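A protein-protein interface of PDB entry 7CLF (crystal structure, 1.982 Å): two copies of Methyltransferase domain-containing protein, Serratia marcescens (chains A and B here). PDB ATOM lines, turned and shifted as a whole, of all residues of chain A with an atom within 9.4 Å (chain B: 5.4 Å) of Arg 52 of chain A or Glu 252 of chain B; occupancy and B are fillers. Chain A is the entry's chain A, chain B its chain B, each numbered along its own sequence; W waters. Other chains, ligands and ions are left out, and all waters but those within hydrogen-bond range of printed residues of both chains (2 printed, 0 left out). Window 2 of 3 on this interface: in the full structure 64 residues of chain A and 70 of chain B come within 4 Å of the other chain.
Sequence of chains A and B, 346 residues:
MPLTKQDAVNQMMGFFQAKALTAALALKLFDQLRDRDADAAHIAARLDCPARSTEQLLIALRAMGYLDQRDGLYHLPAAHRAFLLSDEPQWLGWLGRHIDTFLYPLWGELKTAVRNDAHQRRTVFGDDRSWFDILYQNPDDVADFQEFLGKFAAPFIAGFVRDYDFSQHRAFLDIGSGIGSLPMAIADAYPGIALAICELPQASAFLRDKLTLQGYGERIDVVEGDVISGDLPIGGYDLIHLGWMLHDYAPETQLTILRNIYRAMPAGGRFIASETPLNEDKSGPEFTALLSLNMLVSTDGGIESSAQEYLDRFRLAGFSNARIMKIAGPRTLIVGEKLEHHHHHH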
ATOM      1  N   ALA A  40      12.417 -18.507  14.237  1.00  0.00           N
ATOM      2  CA  ALA A  40      13.569 -18.075  15.024  1.00  0.00           C
ATOM      3  C   ALA A  40      13.827 -19.008  16.196  1.00  0.00           C
ATOM      4  O   ALA A  40      14.979 -19.368  16.462  1.00  0.00           O
ATOM      5  CB  ALA A  40      13.359 -16.644  15.522  1.00  0.00           C
ATOM      6  N   ALA A  41      12.768 -19.398  16.918  1.00  0.00           N
ATOM      7  CA  ALA A  41      12.923 -20.274  18.079  1.00  0.00           C
ATOM      8  C   ALA A  41      13.589 -21.593  17.698  1.00  0.00           C
ATOM      9  O   ALA A  41      14.400 -22.141  18.461  1.00  0.00           O
ATOM     10  CB  ALA A  41      11.558 -20.525  18.716  1.00  0.00           C
ATOM     11  N   ILE A  43      15.542 -22.075  14.900  1.00  0.00           N
ATOM     12  CA  ILE A  43      16.903 -21.797  14.445  1.00  0.00           C
ATOM     13  C   ILE A  43      17.828 -21.597  15.638  1.00  0.00           C
ATOM     14  O   ILE A  43      18.938 -22.136  15.680  1.00  0.00           O
ATOM     15  CB  ILE A  43      16.926 -20.582  13.501  1.00  0.00           C
ATOM     16  CG1 ILE A  43      16.308 -20.926  12.141  1.00  0.00           C
ATOM     17  CG2 ILE A  43      18.353 -20.100  13.285  1.00  0.00           C
ATOM     18  CD1 ILE A  43      15.869 -19.697  11.345  1.00  0.00           C
ATOM     19  N   ALA A  44      17.369 -20.843  16.637  1.00  0.00           N
ATOM     20  CA  ALA A  44      18.169 -20.595  17.831  1.00  0.00           C
ATOM     21  C   ALA A  44      18.487 -21.887  18.566  1.00  0.00           C
ATOM     22  O   ALA A  44      19.633 -22.117  18.976  1.00  0.00           O
ATOM     23  CB  ALA A  44      17.423 -19.635  18.757  1.00  0.00           C
ATOM     24  N   ALA A  45      17.467 -22.726  18.779  1.00  0.00           N
ATOM     25  CA  ALA A  45      17.656 -23.973  19.516  1.00  0.00           C
ATOM     26  C   ALA A  45      18.707 -24.847  18.852  1.00  0.00           C
ATOM     27  O   ALA A  45      19.590 -25.393  19.527  1.00  0.00           O
ATOM     28  CB  ALA A  45      16.328 -24.721  19.636  1.00  0.00           C
ATOM     29  N   CYS A  49      21.742 -21.108  20.642  1.00  0.00           N
ATOM     30  CA  CYS A  49      21.854 -19.685  20.894  1.00  0.00           C
ATOM     31  C   CYS A  49      20.555 -19.193  21.509  1.00  0.00           C
ATOM     32  O   CYS A  49      19.476 -19.703  21.175  1.00  0.00           O
ATOM     33  CB  CYS A  49      22.116 -18.897  19.606  1.00  0.00           C
ATOM     34  SG  CYS A  49      23.773 -18.980  18.925  1.00  0.00           S
ATOM     35  N   PRO A  50      20.615 -18.210  22.407  1.00  0.00           N
ATOM     36  CA  PRO A  50      19.381 -17.668  22.979  1.00  0.00           C
ATOM     37  C   PRO A  50      18.440 -17.226  21.871  1.00  0.00           C
ATOM     38  O   PRO A  50      18.872 -16.719  20.833  1.00  0.00           O
ATOM     39  CB  PRO A  50      19.871 -16.481  23.818  1.00  0.00           C
ATOM     40  CG  PRO A  50      21.290 -16.829  24.143  1.00  0.00           C
ATOM     41  CD  PRO A  50      21.808 -17.526  22.932  1.00  0.00           C
ATOM     42  N   ALA A  51      17.145 -17.460  22.085  1.00  0.00           N
ATOM     43  CA  ALA A  51      16.170 -17.138  21.051  1.00  0.00           C
ATOM     44  C   ALA A  51      16.139 -15.644  20.757  1.00  0.00           C
ATOM     45  O   ALA A  51      15.999 -15.245  19.597  1.00  0.00           O
ATOM     46  CB  ALA A  51      14.780 -17.641  21.453  1.00  0.00           C
ATOM     47  N   ARG A  52      16.292 -14.798  21.786  1.00  0.00           N
ATOM     48  CA  ARG A  52      16.123 -13.363  21.569  1.00  0.00           C
ATOM     49  C   ARG A  52      17.187 -12.818  20.621  1.00  0.00           C
ATOM     50  O   ARG A  52      16.871 -12.113  19.656  1.00  0.00           O
ATOM     51  CB  ARG A  52      16.140 -12.610  22.901  1.00  0.00           C
ATOM     52  CG  ARG A  52      15.901 -11.123  22.753  1.00  0.00           C
ATOM     53  CD  ARG A  52      15.791 -10.453  24.101  1.00  0.00           C
ATOM     54  NE  ARG A  52      14.572 -10.816  24.799  1.00  0.00           N
ATOM     55  CZ  ARG A  52      14.346 -10.547  26.082  1.00  0.00           C
ATOM     56  NH1 ARG A  52      15.269  -9.913  26.798  1.00  0.00           N
ATOM     57  NH2 ARG A  52      13.199 -10.907  26.649  1.00  0.00           N
ATOM     58  N   SER A  53      18.457 -13.173  20.853  1.00  0.00           N
ATOM     59  CA  SER A  53      19.544 -12.626  20.043  1.00  0.00           C
ATOM     60  C   SER A  53      19.643 -13.287  18.669  1.00  0.00           C
ATOM     61  O   SER A  53      20.009 -12.625  17.689  1.00  0.00           O
ATOM     62  CB  SER A  53      20.867 -12.771  20.790  1.00  0.00           C
ATOM     63  OG  SER A  53      20.958 -14.068  21.342  1.00  0.00           O
ATOM     64  N   THR A  54      19.334 -14.580  18.570  1.00  0.00           N
ATOM     65  CA  THR A  54      19.219 -15.199  17.254  1.00  0.00           C
ATOM     66  C   THR A  54      18.167 -14.498  16.409  1.00  0.00           C
ATOM     67  O   THR A  54      18.374 -14.262  15.213  1.00  0.00           O
ATOM     68  CB  THR A  54      18.859 -16.671  17.395  1.00  0.00           C
ATOM     69  OG1 THR A  54      19.867 -17.315  18.169  1.00  0.00           O
ATOM     70  CG2 THR A  54      18.761 -17.326  16.021  1.00  0.00           C
ATOM     71  N   GLU A  55      17.029 -14.165  17.022  1.00  0.00           N
ATOM     72  CA  GLU A  55      15.953 -13.491  16.302  1.00  0.00           C
ATOM     73  C   GLU A  55      16.378 -12.101  15.859  1.00  0.00           C
ATOM     74  O   GLU A  55      16.030 -11.658  14.756  1.00  0.00           O
ATOM     75  CB  GLU A  55      14.696 -13.409  17.173  1.00  0.00           C
ATOM     76  CG  GLU A  55      13.537 -12.682  16.463  1.00  0.00           C
ATOM     77  CD  GLU A  55      12.187 -12.818  17.144  1.00  0.00           C
ATOM     78  OE1 GLU A  55      12.097 -12.631  18.373  1.00  0.00           O
ATOM     79  OE2 GLU A  55      11.197 -13.110  16.437  1.00  0.00           O
ATOM     80  N   GLN A  56      17.127 -11.393  16.712  1.00  0.00           N
ATOM     81  CA  GLN A  56      17.620 -10.079  16.325  1.00  0.00           C
ATOM     82  C   GLN A  56      18.465 -10.168  15.065  1.00  0.00           C
ATOM     83  O   GLN A  56      18.334  -9.334  14.159  1.00  0.00           O
ATOM     84  CB  GLN A  56      18.420  -9.448  17.476  1.00  0.00           C
ATOM     85  CG  GLN A  56      17.559  -8.988  18.655  1.00  0.00           C
ATOM     86  CD  GLN A  56      18.383  -8.448  19.825  1.00  0.00           C
ATOM     87  OE1 GLN A  56      18.813  -9.203  20.696  1.00  0.00           O
ATOM     88  NE2 GLN A  56      18.599  -7.139  19.846  1.00  0.00           N
ATOM     89  N   LEU A  57      19.339 -11.178  14.984  1.00  0.00           N
ATOM     90  CA  LEU A  57      20.161 -11.327  13.790  1.00  0.00           C
ATOM     91  C   LEU A  57      19.316 -11.737  12.589  1.00  0.00           C
ATOM     92  O   LEU A  57      19.514 -11.226  11.480  1.00  0.00           O
ATOM     93  CB  LEU A  57      21.278 -12.346  14.032  1.00  0.00           C
ATOM     94  CG  LEU A  57      22.055 -12.745  12.779  1.00  0.00           C
ATOM     95  CD1 LEU A  57      22.637 -11.493  12.100  1.00  0.00           C
ATOM     96  CD2 LEU A  57      23.182 -13.736  13.125  1.00  0.00           C
ATOM     97  N   LEU A  58      18.385 -12.671  12.794  1.00  0.00           N
ATOM     98  CA  LEU A  58      17.505 -13.111  11.712  1.00  0.00           C
ATOM     99  C   LEU A  58      16.651 -11.966  11.172  1.00  0.00           C
ATOM    100  O   LEU A  58      16.467 -11.844   9.956  1.00  0.00           O
ATOM    101  CB  LEU A  58      16.621 -14.255  12.204  1.00  0.00           C
ATOM    102  CG  LEU A  58      17.291 -15.610  12.446  1.00  0.00           C
ATOM    103  CD1 LEU A  58      16.396 -16.470  13.307  1.00  0.00           C
ATOM    104  CD2 LEU A  58      17.616 -16.316  11.127  1.00  0.00           C
ATOM    105  N   ILE A  59      16.106 -11.123  12.056  1.00  0.00           N
ATOM    106  CA  ILE A  59      15.306  -9.989  11.585  1.00  0.00           C
ATOM    107  C   ILE A  59      16.163  -9.046  10.747  1.00  0.00           C
ATOM    108  O   ILE A  59      15.707  -8.508   9.730  1.00  0.00           O
ATOM    109  CB  ILE A  59      14.640  -9.271  12.778  1.00  0.00           C
ATOM    110  CG1 ILE A  59      13.490 -10.120  13.337  1.00  0.00           C
ATOM    111  CG2 ILE A  59      14.179  -7.834  12.396  1.00  0.00           C
ATOM    112  CD1 ILE A  59      13.055  -9.704  14.746  1.00  0.00           C
ATOM    113  N   ALA A  60      17.433  -8.860  11.134  1.00  0.00           N
ATOM    114  CA  ALA A  60      18.313  -7.980  10.366  1.00  0.00           C
ATOM    115  C   ALA A  60      18.594  -8.549   8.982  1.00  0.00           C
ATOM    116  O   ALA A  60      18.583  -7.811   7.991  1.00  0.00           O
ATOM    117  CB  ALA A  60      19.625  -7.735  11.125  1.00  0.00           C
ATOM    118  N   TYR A  74      11.340 -18.433   8.540  1.00  0.00           N
ATOM    119  CA  TYR A  74      12.436 -17.947   7.662  1.00  0.00           C
ATOM    120  C   TYR A  74      12.691 -18.942   6.529  1.00  0.00           C
ATOM    121  O   TYR A  74      12.570 -20.138   6.754  1.00  0.00           O
ATOM    122  CB  TYR A  74      13.708 -17.613   8.439  1.00  0.00           C
ATOM    123  CG  TYR A  74      13.537 -16.423   9.331  1.00  0.00           C
ATOM    124  CD1 TYR A  74      13.012 -16.569  10.591  1.00  0.00           C
ATOM    125  CD2 TYR A  74      13.813 -15.149   8.884  1.00  0.00           C
ATOM    126  CE1 TYR A  74      12.781 -15.486  11.403  1.00  0.00           C
ATOM    127  CE2 TYR A  74      13.610 -14.050   9.692  1.00  0.00           C
ATOM    128  CZ  TYR A  74      13.087 -14.224  10.956  1.00  0.00           C
ATOM    129  OH  TYR A  74      12.890 -13.168  11.767  1.00  0.00           O
ATOM    130  N   ASP B 117      23.656 -13.767  23.800  1.00  0.00           N
ATOM    131  CA  ASP B 117      22.670 -12.714  24.052  1.00  0.00           C
ATOM    132  C   ASP B 117      23.170 -11.764  25.133  1.00  0.00           C
ATOM    133  O   ASP B 117      22.534 -11.555  26.166  1.00  0.00           O
ATOM    134  CB  ASP B 117      21.303 -13.292  24.420  1.00  0.00           C
ATOM    135  CG  ASP B 117      20.216 -12.218  24.498  1.00  0.00           C
ATOM    136  OD1 ASP B 117      20.412 -11.137  23.894  1.00  0.00           O
ATOM    137  OD2 ASP B 117      19.190 -12.442  25.181  1.00  0.00           O
ATOM    138  N   ALA B 250      16.258  -4.067  28.252  1.00  0.00           N
ATOM    139  CA  ALA B 250      15.485  -5.264  27.982  1.00  0.00           C
ATOM    140  C   ALA B 250      14.000  -5.020  28.259  1.00  0.00           C
ATOM    141  O   ALA B 250      13.645  -4.255  29.159  1.00  0.00           O
ATOM    142  CB  ALA B 250      15.986  -6.420  28.836  1.00  0.00           C
ATOM    143  N   PRO B 251      13.113  -5.684  27.505  1.00  0.00           N
ATOM    144  CA  PRO B 251      11.667  -5.555  27.740  1.00  0.00           C
ATOM    145  C   PRO B 251      11.275  -5.562  29.206  1.00  0.00           C
ATOM    146  O   PRO B 251      10.493  -4.723  29.666  1.00  0.00           O
ATOM    147  CB  PRO B 251      11.105  -6.793  27.029  1.00  0.00           C
ATOM    148  CG  PRO B 251      12.052  -7.026  25.924  1.00  0.00           C
ATOM    149  CD  PRO B 251      13.408  -6.684  26.465  1.00  0.00           C
ATOM    150  N   GLU B 252      11.815  -6.544  29.927  1.00  0.00           N
ATOM    151  CA  GLU B 252      11.604  -6.643  31.368  1.00  0.00           C
ATOM    152  C   GLU B 252      11.971  -5.349  32.076  1.00  0.00           C
ATOM    153  O   GLU B 252      11.272  -4.919  33.003  1.00  0.00           O
ATOM    154  CB  GLU B 252      12.426  -7.808  31.928  1.00  0.00           C
ATOM    155  CG  GLU B 252      12.098  -9.165  31.310  1.00  0.00           C
ATOM    156  CD  GLU B 252      12.704  -9.367  29.916  1.00  0.00           C
ATOM    157  OE1 GLU B 252      12.093 -10.105  29.108  1.00  0.00           O
ATOM    158  OE2 GLU B 252      13.781  -8.809  29.631  1.00  0.00           O
ATOM    159  N   THR B 253      13.066  -4.712  31.660  1.00  0.00           N
ATOM    160  CA  THR B 253      13.460  -3.447  32.269  1.00  0.00           C
ATOM    161  C   THR B 253      12.593  -2.287  31.781  1.00  0.00           C
ATOM    162  O   THR B 253      12.337  -1.341  32.539  1.00  0.00           O
ATOM    163  CB  THR B 253      14.937  -3.176  31.980  1.00  0.00           C
ATOM    164  OG1 THR B 253      15.737  -4.253  32.493  1.00  0.00           O
ATOM    165  CG2 THR B 253      15.371  -1.877  32.616  1.00  0.00           C
ATOM    166  N   GLN B 254      12.135  -2.337  30.528  1.00  0.00           N
ATOM    167  CA  GLN B 254      11.220  -1.310  30.055  1.00  0.00           C
ATOM    168  C   GLN B 254       9.938  -1.322  30.866  1.00  0.00           C
ATOM    169  O   GLN B 254       9.359  -0.260  31.134  1.00  0.00           O
ATOM    170  CB  GLN B 254      10.910  -1.515  28.580  1.00  0.00           C
ATOM    171  CG  GLN B 254      12.137  -1.607  27.711  1.00  0.00           C
ATOM    172  CD  GLN B 254      11.773  -1.814  26.258  1.00  0.00           C
ATOM    173  OE1 GLN B 254      10.692  -1.406  25.804  1.00  0.00           O
ATOM    174  NE2 GLN B 254      12.646  -2.481  25.525  1.00  0.00           N
ATOM    175  N   LEU B 255       9.495  -2.514  31.275  1.00  0.00           N
ATOM    176  CA  LEU B 255       8.351  -2.639  32.169  1.00  0.00           C
ATOM    177  C   LEU B 255       8.560  -1.816  33.431  1.00  0.00           C
ATOM    178  O   LEU B 255       7.689  -1.020  33.810  1.00  0.00           O
ATOM    179  CB  LEU B 255       8.113  -4.118  32.503  1.00  0.00           C
ATOM    180  CG  LEU B 255       7.203  -4.877  31.532  1.00  0.00           C
ATOM    181  CD1 LEU B 255       6.840  -6.263  32.069  1.00  0.00           C
ATOM    182  CD2 LEU B 255       5.941  -4.085  31.195  1.00  0.00           C
ATOM    183  N   THR B 256       9.724  -1.980  34.080  1.00  0.00           N
ATOM    184  CA  THR B 256      10.026  -1.212  35.284  1.00  0.00           C
ATOM    185  C   THR B 256       9.999   0.289  35.000  1.00  0.00           C
ATOM    186  O   THR B 256       9.423   1.070  35.770  1.00  0.00           O
ATOM    187  CB  THR B 256      11.384  -1.630  35.845  1.00  0.00           C
ATOM    188  OG1 THR B 256      11.402  -3.041  36.077  1.00  0.00           O
ATOM    189  CG2 THR B 256      11.667  -0.904  37.158  1.00  0.00           C
ATOM    190  N   GLY B 301      20.966  -4.981  27.565  1.00  0.00           N
ATOM    191  CA  GLY B 301      19.776  -5.704  27.162  1.00  0.00           C
ATOM    192  C   GLY B 301      18.938  -5.071  26.072  1.00  0.00           C
ATOM    193  O   GLY B 301      17.829  -5.555  25.817  1.00  0.00           O
ATOM    194  N   ILE B 303      17.151  -3.649  22.585  1.00  0.00           N
ATOM    195  CA  ILE B 303      16.529  -4.350  21.465  1.00  0.00           C
ATOM    196  C   ILE B 303      15.452  -3.435  20.893  1.00  0.00           C
ATOM    197  O   ILE B 303      14.897  -2.589  21.615  1.00  0.00           O
ATOM    198  CB  ILE B 303      15.949  -5.707  21.924  1.00  0.00           C
ATOM    199  CG1 ILE B 303      15.205  -6.444  20.783  1.00  0.00           C
ATOM    200  CG2 ILE B 303      15.008  -5.510  23.105  1.00  0.00           C
ATOM    201  CD1 ILE B 303      15.059  -7.948  21.004  1.00  0.00           C
HETATM  202  O   HOH W   1      18.925  -9.077  23.573  1.00  0.00           O
HETATM  203  O   HOH W   2      17.540  -8.333  25.670  1.00  0.00           O
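Among the printed residues, merely in contact across the chains: Ser 53 of chain A with Asp 117 of chain B, Pro 50 of chain A with Asp 117 of chain B, Gln 56 of chain A with Ile 303 of chain B, Arg 52 of chain A with Ile 303 of chain B, Arg 52 of chain A with Pro 251 of chain B and Arg 52 of chain A with Asp 117 of chain B.
Water W1 bridges OD1 of Asp 117 of chain B and OE1 of Gln 56 of chain A. Water W2 lies within hydrogen-bond range of O of Gly 301 of chain B (2.8 Å) and NH1 of Arg 52 of chain A (3.0 Å).
No position is printed for both chains. Of the 7 pairs that touch across the chains among the printed residues, none has its exchanged pair printed and touching as well.
O of Pro 50 of chain A sits at hydrogen-bond distance from OG of Ser 53 of chain A (3.4 Å). OG1 of Thr 54 of chain A lies within hydrogen-bond range of O of Pro 50 of chain A.
NH2 of Arg 52 of chain A lies within salt-bridge range of OE1 of Glu 252 of chain B (2.8 Å).
Of the printed residues of chain B, Pro 50 of chain A touches Asp 117. Arg 52 of chain A touches four residues of chain B. Printed residues of chain B within 4 Å of Ser 53 of chain A: Asp 117 (3.2 Å). Printed residues of chain B within 4 Å of Gln 56 of chain A: Ile 303. Printed residues of chain A within 4 Å of Asp 117 of chain B: Pro 50 (3.5 Å), Arg 52 (3.8 Å) and Ser 53 (3.2 Å). Of chain A, only Arg 52 comes within 4 Å of Glu 252 of chain B. No residue of chain A comes within 4 Å of Thr 253 of chain B. Of the printed residues of chain A, Ile 303 of chain B touches Arg 52 and Gln 56. The nearest printed residue of chain A that does not touch Glu 252 of chain B is Gln 56 of chain A (10.3 Å). The nearest printed residue of chain B that does not touch Ser 53 of chain A is Ile 303 of chain B (6.2 Å).
Printed residues of chain A that touch a printed residue of chain B: Pro 50, Arg 52, Ser 53 and Gln 56. Among the printed residues, 7 pairs touch across the chains. Among the printed residues, Asp or Glu carboxylates within 4 Å of a Lys or Arg side-chain nitrogen of the other chain: Arg 52 of chain A with Glu 252 of chain B (2.8 Å).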
